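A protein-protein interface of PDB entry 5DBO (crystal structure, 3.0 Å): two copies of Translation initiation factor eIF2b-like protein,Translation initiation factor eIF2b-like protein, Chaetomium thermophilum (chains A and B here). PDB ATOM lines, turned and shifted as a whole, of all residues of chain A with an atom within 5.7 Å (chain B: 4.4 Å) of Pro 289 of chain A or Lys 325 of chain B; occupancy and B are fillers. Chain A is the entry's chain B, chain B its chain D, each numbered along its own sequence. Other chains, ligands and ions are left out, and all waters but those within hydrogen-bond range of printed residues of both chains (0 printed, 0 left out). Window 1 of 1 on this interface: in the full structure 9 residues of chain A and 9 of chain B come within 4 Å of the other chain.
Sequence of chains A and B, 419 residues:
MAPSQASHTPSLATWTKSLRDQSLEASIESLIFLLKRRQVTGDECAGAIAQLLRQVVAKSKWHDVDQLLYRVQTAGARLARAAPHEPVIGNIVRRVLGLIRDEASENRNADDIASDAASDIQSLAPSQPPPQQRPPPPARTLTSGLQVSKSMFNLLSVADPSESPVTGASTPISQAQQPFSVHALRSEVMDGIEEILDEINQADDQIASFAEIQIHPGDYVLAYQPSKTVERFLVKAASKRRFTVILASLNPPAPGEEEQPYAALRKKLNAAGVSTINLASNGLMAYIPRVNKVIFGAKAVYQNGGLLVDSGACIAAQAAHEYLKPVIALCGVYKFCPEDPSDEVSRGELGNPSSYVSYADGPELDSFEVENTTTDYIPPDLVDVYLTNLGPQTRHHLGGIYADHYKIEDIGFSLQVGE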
ATOM      1  N   LEU A 284      -5.013   9.516 -16.502  1.00  0.00           N
ATOM      2  CA  LEU A 284      -5.521   9.289 -17.850  1.00  0.00           C
ATOM      3  C   LEU A 284      -4.803  10.143 -18.872  1.00  0.00           C
ATOM      4  O   LEU A 284      -5.193  10.188 -20.040  1.00  0.00           O
ATOM      5  CB  LEU A 284      -7.025   9.574 -17.922  1.00  0.00           C
ATOM      6  CG  LEU A 284      -8.058   8.595 -17.364  1.00  0.00           C
ATOM      7  CD1 LEU A 284      -7.660   7.953 -16.044  1.00  0.00           C
ATOM      8  CD2 LEU A 284      -9.366   9.347 -17.207  1.00  0.00           C
ATOM      9  N   MET A 285      -3.758  10.828 -18.425  1.00  0.00           N
ATOM     10  CA  MET A 285      -3.023  11.746 -19.282  1.00  0.00           C
ATOM     11  C   MET A 285      -2.433  11.056 -20.504  1.00  0.00           C
ATOM     12  O   MET A 285      -2.380  11.637 -21.591  1.00  0.00           O
ATOM     13  CB  MET A 285      -1.911  12.422 -18.491  1.00  0.00           C
ATOM     14  CG  MET A 285      -1.352  13.633 -19.194  1.00  0.00           C
ATOM     15  SD  MET A 285      -2.626  14.894 -19.232  1.00  0.00           S
ATOM     16  CE  MET A 285      -3.182  14.799 -17.527  1.00  0.00           C
ATOM     17  N   ALA A 286      -2.010   9.809 -20.325  1.00  0.00           N
ATOM     18  CA  ALA A 286      -1.412   9.047 -21.412  1.00  0.00           C
ATOM     19  C   ALA A 286      -2.429   8.780 -22.516  1.00  0.00           C
ATOM     20  O   ALA A 286      -2.077   8.766 -23.698  1.00  0.00           O
ATOM     21  CB  ALA A 286      -0.834   7.737 -20.891  1.00  0.00           C
ATOM     22  N   TYR A 287      -3.685   8.565 -22.128  1.00  0.00           N
ATOM     23  CA  TYR A 287      -4.707   8.119 -23.075  1.00  0.00           C
ATOM     24  C   TYR A 287      -5.618   9.227 -23.633  1.00  0.00           C
ATOM     25  O   TYR A 287      -6.271   9.027 -24.657  1.00  0.00           O
ATOM     26  CB  TYR A 287      -5.571   7.032 -22.422  1.00  0.00           C
ATOM     27  CG  TYR A 287      -4.791   6.046 -21.567  1.00  0.00           C
ATOM     28  CD1 TYR A 287      -4.203   4.918 -22.132  1.00  0.00           C
ATOM     29  CD2 TYR A 287      -4.663   6.232 -20.196  1.00  0.00           C
ATOM     30  CE1 TYR A 287      -3.494   4.013 -21.358  1.00  0.00           C
ATOM     31  CE2 TYR A 287      -3.961   5.335 -19.414  1.00  0.00           C
ATOM     32  CZ  TYR A 287      -3.377   4.223 -19.998  1.00  0.00           C
ATOM     33  OH  TYR A 287      -2.669   3.322 -19.222  1.00  0.00           O
ATOM     34  N   ILE A 288      -5.666  10.382 -22.973  1.00  0.00           N
ATOM     35  CA  ILE A 288      -6.567  11.471 -23.380  1.00  0.00           C
ATOM     36  C   ILE A 288      -6.443  12.006 -24.820  1.00  0.00           C
ATOM     37  O   ILE A 288      -7.464  12.242 -25.468  1.00  0.00           O
ATOM     38  CB  ILE A 288      -6.434  12.670 -22.414  1.00  0.00           C
ATOM     39  CG1 ILE A 288      -7.307  12.424 -21.192  1.00  0.00           C
ATOM     40  CG2 ILE A 288      -6.939  13.952 -23.046  1.00  0.00           C
ATOM     41  CD1 ILE A 288      -8.790  12.400 -21.521  1.00  0.00           C
ATOM     42  N   PRO A 289      -5.214  12.202 -25.335  1.00  0.00           N
ATOM     43  CA  PRO A 289      -5.135  12.755 -26.695  1.00  0.00           C
ATOM     44  C   PRO A 289      -5.825  11.889 -27.746  1.00  0.00           C
ATOM     45  O   PRO A 289      -6.276  12.388 -28.777  1.00  0.00           O
ATOM     46  CB  PRO A 289      -3.626  12.826 -26.951  1.00  0.00           C
ATOM     47  CG  PRO A 289      -3.040  11.861 -25.993  1.00  0.00           C
ATOM     48  CD  PRO A 289      -3.870  11.998 -24.773  1.00  0.00           C
ATOM     49  N   ARG A 290      -5.898  10.594 -27.469  1.00  0.00           N
ATOM     50  CA  ARG A 290      -6.496   9.629 -28.378  1.00  0.00           C
ATOM     51  C   ARG A 290      -8.028   9.648 -28.375  1.00  0.00           C
ATOM     52  O   ARG A 290      -8.645   9.328 -29.388  1.00  0.00           O
ATOM     53  CB  ARG A 290      -5.989   8.229 -28.030  1.00  0.00           C
ATOM     54  CG  ARG A 290      -4.498   8.020 -28.300  1.00  0.00           C
ATOM     55  CD  ARG A 290      -4.176   8.031 -29.778  1.00  0.00           C
ATOM     56  NE  ARG A 290      -4.691   6.828 -30.428  1.00  0.00           N
ATOM     57  CZ  ARG A 290      -4.571   6.563 -31.724  1.00  0.00           C
ATOM     58  NH1 ARG A 290      -3.939   7.414 -32.522  1.00  0.00           N
ATOM     59  NH2 ARG A 290      -5.075   5.440 -32.221  1.00  0.00           N
ATOM     60  N   VAL A 291      -8.637   9.997 -27.240  1.00  0.00           N
ATOM     61  CA  VAL A 291     -10.104  10.092 -27.142  1.00  0.00           C
ATOM     62  C   VAL A 291     -10.648  11.391 -27.732  1.00  0.00           C
ATOM     63  O   VAL A 291      -9.944  12.398 -27.806  1.00  0.00           O
ATOM     64  CB  VAL A 291     -10.615   9.998 -25.683  1.00  0.00           C
ATOM     65  CG1 VAL A 291      -9.947   8.850 -24.952  1.00  0.00           C
ATOM     66  CG2 VAL A 291     -10.386  11.302 -24.943  1.00  0.00           C
ATOM     67  N   TYR A 323      -6.406  19.289 -23.302  1.00  0.00           N
ATOM     68  CA  TYR A 323      -6.292  18.895 -24.701  1.00  0.00           C
ATOM     69  C   TYR A 323      -7.476  19.392 -25.516  1.00  0.00           C
ATOM     70  O   TYR A 323      -7.641  19.023 -26.682  1.00  0.00           O
ATOM     71  CB  TYR A 323      -6.131  17.376 -24.822  1.00  0.00           C
ATOM     72  CG  TYR A 323      -4.715  16.952 -24.495  1.00  0.00           C
ATOM     73  CD1 TYR A 323      -3.740  16.906 -25.486  1.00  0.00           C
ATOM     74  CD2 TYR A 323      -4.334  16.674 -23.186  1.00  0.00           C
ATOM     75  CE1 TYR A 323      -2.439  16.550 -25.195  1.00  0.00           C
ATOM     76  CE2 TYR A 323      -3.027  16.311 -22.883  1.00  0.00           C
ATOM     77  CZ  TYR A 323      -2.082  16.254 -23.894  1.00  0.00           C
ATOM     78  OH  TYR A 323      -0.779  15.897 -23.609  1.00  0.00           O
ATOM     79  N   LYS A 325     -10.509  18.719 -25.200  1.00  0.00           N
ATOM     80  CA  LYS A 325     -11.520  17.684 -25.404  1.00  0.00           C
ATOM     81  C   LYS A 325     -12.817  18.073 -24.703  1.00  0.00           C
ATOM     82  O   LYS A 325     -12.799  18.444 -23.529  1.00  0.00           O
ATOM     83  CB  LYS A 325     -11.032  16.336 -24.867  1.00  0.00           C
ATOM     84  CG  LYS A 325      -9.669  15.904 -25.377  1.00  0.00           C
ATOM     85  CD  LYS A 325      -9.684  15.736 -26.881  1.00  0.00           C
ATOM     86  CE  LYS A 325      -8.418  15.064 -27.379  1.00  0.00           C
ATOM     87  NZ  LYS A 325      -8.602  14.601 -28.782  1.00  0.00           N
ATOM     88  N   ILE B 288      -9.126  19.444 -37.363  1.00  0.00           N
ATOM     89  CA  ILE B 288      -7.950  19.215 -36.518  1.00  0.00           C
ATOM     90  C   ILE B 288      -8.155  18.317 -35.281  1.00  0.00           C
ATOM     91  O   ILE B 288      -7.321  17.445 -35.020  1.00  0.00           O
ATOM     92  CB  ILE B 288      -7.364  20.561 -36.041  1.00  0.00           C
ATOM     93  CG1 ILE B 288      -6.555  21.189 -37.163  1.00  0.00           C
ATOM     94  CG2 ILE B 288      -6.460  20.372 -34.842  1.00  0.00           C
ATOM     95  CD1 ILE B 288      -5.323  20.377 -37.515  1.00  0.00           C
ATOM     96  N   PRO B 289      -9.257  18.494 -34.527  1.00  0.00           N
ATOM     97  CA  PRO B 289      -9.380  17.638 -33.341  1.00  0.00           C
ATOM     98  C   PRO B 289      -9.407  16.139 -33.651  1.00  0.00           C
ATOM     99  O   PRO B 289      -9.022  15.342 -32.790  1.00  0.00           O
ATOM    100  CB  PRO B 289     -10.699  18.103 -32.715  1.00  0.00           C
ATOM    101  CG  PRO B 289     -11.429  18.784 -33.827  1.00  0.00           C
ATOM    102  CD  PRO B 289     -10.356  19.472 -34.587  1.00  0.00           C
ATOM    103  N   VAL B 291      -7.651  14.539 -36.175  1.00  0.00           N
ATOM    104  CA  VAL B 291      -6.324  14.014 -36.516  1.00  0.00           C
ATOM    105  C   VAL B 291      -5.458  13.892 -35.263  1.00  0.00           C
ATOM    106  O   VAL B 291      -5.680  14.592 -34.278  1.00  0.00           O
ATOM    107  CB  VAL B 291      -5.584  14.893 -37.555  1.00  0.00           C
ATOM    108  CG1 VAL B 291      -6.487  15.221 -38.732  1.00  0.00           C
ATOM    109  CG2 VAL B 291      -5.049  16.157 -36.917  1.00  0.00           C
ATOM    110  N   ASN B 292      -4.471  13.006 -35.296  1.00  0.00           N
ATOM    111  CA  ASN B 292      -3.577  12.842 -34.152  1.00  0.00           C
ATOM    112  C   ASN B 292      -2.272  13.600 -34.305  1.00  0.00           C
ATOM    113  O   ASN B 292      -1.674  14.003 -33.310  1.00  0.00           O
ATOM    114  CB  ASN B 292      -3.274  11.365 -33.900  1.00  0.00           C
ATOM    115  CG  ASN B 292      -4.481  10.607 -33.411  1.00  0.00           C
ATOM    116  OD1 ASN B 292      -4.958   9.679 -34.063  1.00  0.00           O
ATOM    117  ND2 ASN B 292      -5.002  11.018 -32.258  1.00  0.00           N
ATOM    118  N   ALA B 320      -3.173  23.070 -35.413  1.00  0.00           N
ATOM    119  CA  ALA B 320      -2.645  21.900 -34.717  1.00  0.00           C
ATOM    120  C   ALA B 320      -2.075  22.273 -33.357  1.00  0.00           C
ATOM    121  O   ALA B 320      -2.264  21.559 -32.370  1.00  0.00           O
ATOM    122  CB  ALA B 320      -1.577  21.225 -35.552  1.00  0.00           C
ATOM    123  N   TYR B 323      -4.589  22.750 -30.474  1.00  0.00           N
ATOM    124  CA  TYR B 323      -5.175  21.523 -29.953  1.00  0.00           C
ATOM    125  C   TYR B 323      -4.092  20.568 -29.457  1.00  0.00           C
ATOM    126  O   TYR B 323      -4.367  19.399 -29.179  1.00  0.00           O
ATOM    127  CB  TYR B 323      -6.054  20.836 -31.006  1.00  0.00           C
ATOM    128  CG  TYR B 323      -7.426  21.468 -31.150  1.00  0.00           C
ATOM    129  CD1 TYR B 323      -7.640  22.528 -32.020  1.00  0.00           C
ATOM    130  CD2 TYR B 323      -8.491  21.039 -30.369  1.00  0.00           C
ATOM    131  CE1 TYR B 323      -8.884  23.108 -32.139  1.00  0.00           C
ATOM    132  CE2 TYR B 323      -9.736  21.619 -30.476  1.00  0.00           C
ATOM    133  CZ  TYR B 323      -9.930  22.654 -31.362  1.00  0.00           C
ATOM    134  OH  TYR B 323     -11.176  23.237 -31.474  1.00  0.00           O
ATOM    135  N   LEU B 324      -2.865  21.078 -29.361  1.00  0.00           N
ATOM    136  CA  LEU B 324      -1.720  20.314 -28.869  1.00  0.00           C
ATOM    137  C   LEU B 324      -1.486  19.036 -29.663  1.00  0.00           C
ATOM    138  O   LEU B 324      -1.037  18.021 -29.120  1.00  0.00           O
ATOM    139  CB  LEU B 324      -1.862  19.983 -27.382  1.00  0.00           C
ATOM    140  CG  LEU B 324      -1.373  21.037 -26.386  1.00  0.00           C
ATOM    141  CD1 LEU B 324      -2.056  22.368 -26.594  1.00  0.00           C
ATOM    142  CD2 LEU B 324      -1.567  20.549 -24.958  1.00  0.00           C
ATOM    143  N   LYS B 325      -1.785  19.093 -30.954  1.00  0.00           N
ATOM    144  CA  LYS B 325      -1.434  18.003 -31.846  1.00  0.00           C
ATOM    145  C   LYS B 325       0.019  18.208 -32.264  1.00  0.00           C
ATOM    146  O   LYS B 325       0.403  19.311 -32.655  1.00  0.00           O
ATOM    147  CB  LYS B 325      -2.363  17.965 -33.063  1.00  0.00           C
ATOM    148  CG  LYS B 325      -3.855  17.941 -32.723  1.00  0.00           C
ATOM    149  CD  LYS B 325      -4.214  16.700 -31.926  1.00  0.00           C
ATOM    150  CE  LYS B 325      -5.718  16.515 -31.802  1.00  0.00           C
ATOM    151  NZ  LYS B 325      -6.062  15.136 -31.337  1.00  0.00           N
ATOM    152  N   PRO B 326       0.836  17.153 -32.155  1.00  0.00           N
ATOM    153  CA  PRO B 326       2.256  17.226 -32.522  1.00  0.00           C
ATOM    154  C   PRO B 326       2.473  17.640 -33.974  1.00  0.00           C
ATOM    155  O   PRO B 326       1.823  17.118 -34.892  1.00  0.00           O
ATOM    156  CB  PRO B 326       2.756  15.799 -32.273  1.00  0.00           C
ATOM    157  CG  PRO B 326       1.872  15.293 -31.193  1.00  0.00           C
ATOM    158  CD  PRO B 326       0.510  15.881 -31.490  1.00  0.00           C
ATOM    159  N   VAL B 327       3.362  18.611 -34.162  1.00  0.00           N
ATOM    160  CA  VAL B 327       3.736  19.067 -35.492  1.00  0.00           C
ATOM    161  C   VAL B 327       5.120  18.551 -35.873  1.00  0.00           C
ATOM    162  O   VAL B 327       6.127  18.856 -35.223  1.00  0.00           O
ATOM    163  CB  VAL B 327       3.719  20.604 -35.598  1.00  0.00           C
ATOM    164  CG1 VAL B 327       4.367  21.052 -36.901  1.00  0.00           C
ATOM    165  CG2 VAL B 327       2.295  21.131 -35.489  1.00  0.00           C
ATOM    166  N   ASP B 384       6.994  21.028 -33.184  1.00  0.00           N
ATOM    167  CA  ASP B 384       7.401  20.197 -32.058  1.00  0.00           C
ATOM    168  C   ASP B 384       8.496  19.178 -32.366  1.00  0.00           C
ATOM    169  O   ASP B 384       9.250  18.800 -31.467  1.00  0.00           O
ATOM    170  CB  ASP B 384       6.184  19.482 -31.481  1.00  0.00           C
ATOM    171  CG  ASP B 384       5.075  20.440 -31.133  1.00  0.00           C
ATOM    172  OD1 ASP B 384       5.300  21.304 -30.257  1.00  0.00           O
ATOM    173  OD2 ASP B 384       3.987  20.336 -31.736  1.00  0.00           O
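O of Pro 289 of chain A is in hydrogen-bond range of NZ of Lys 325 of chain A (3.2 Å).
The side-chain amino group of Lys 325 of chain B sits at hydrogen-bond distance from the backbone carbonyl oxygen of Val 291 of chain B (3.0 Å).
The backbone NH (N) of Lys 325 of chain B sits at hydrogen-bond distance from the backbone carbonyl oxygen (O) of Ala 320 of chain B, at 2.9 Å.
The backbone carbonyl oxygen (O) of Val 291 of chain A lies within hydrogen-bond range of the side-chain amino group (NZ) of Lys 325 of chain A (2.8 Å).
The backbone carbonyl oxygen (O) of Pro 289 of chain B is in hydrogen-bond range of the side-chain amino group (NZ) of Lys 325 of chain B, 3.3 Å away.
NH1 of Arg 290 of chain A sits at hydrogen-bond distance from OD1 of Asn 292 of chain B (2.9 Å).
Pro 289 of chain A touches Lys 325 of chain B, but with the chains exchanged Lys 325 of chain A does not touch Pro 289 of chain B (4.1 Å).
Lys 325 of chain B touches its own counterpart, Lys 325 of chain A.
Asn 292 of chain B touches Pro 289 of chain A.
Pro 289 of chain A touches Lys 325 of chain B.
Lys 325 of chain B touches Lys 325 of chain A (NZ to NZ, 3.6 Å).
Among the printed residues, no Asp or Glu carboxylate lies within 4 Å of a Lys or Arg side-chain nitrogen of the other chain.
Pro 289 of chain A touches just these residues of chain B: Asn 292 (3.95 Å) and Lys 325 (3.8 Å).
Printed residues of chain B within 4 Å of Arg 290 of chain A: Asn 292 (2.9 Å).
Ile 288 of chain B touches none of the printed residues of chain A.
Pro 289 of chain B touches none of the printed residues of chain A.
Printed residues of chain A within 4 Å of Asn 292 of chain B: Pro 289 (3.95 Å) and Arg 290 (2.9 Å).
Of chain A, only Pro 289 (3.8 Å) and Lys 325 (3.6 Å) come within 4 Å of Lys 325 of chain B.
The nearest printed residue of chain B that does not touch Arg 290 of chain A is Lys 325 of chain B (6.0 Å).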
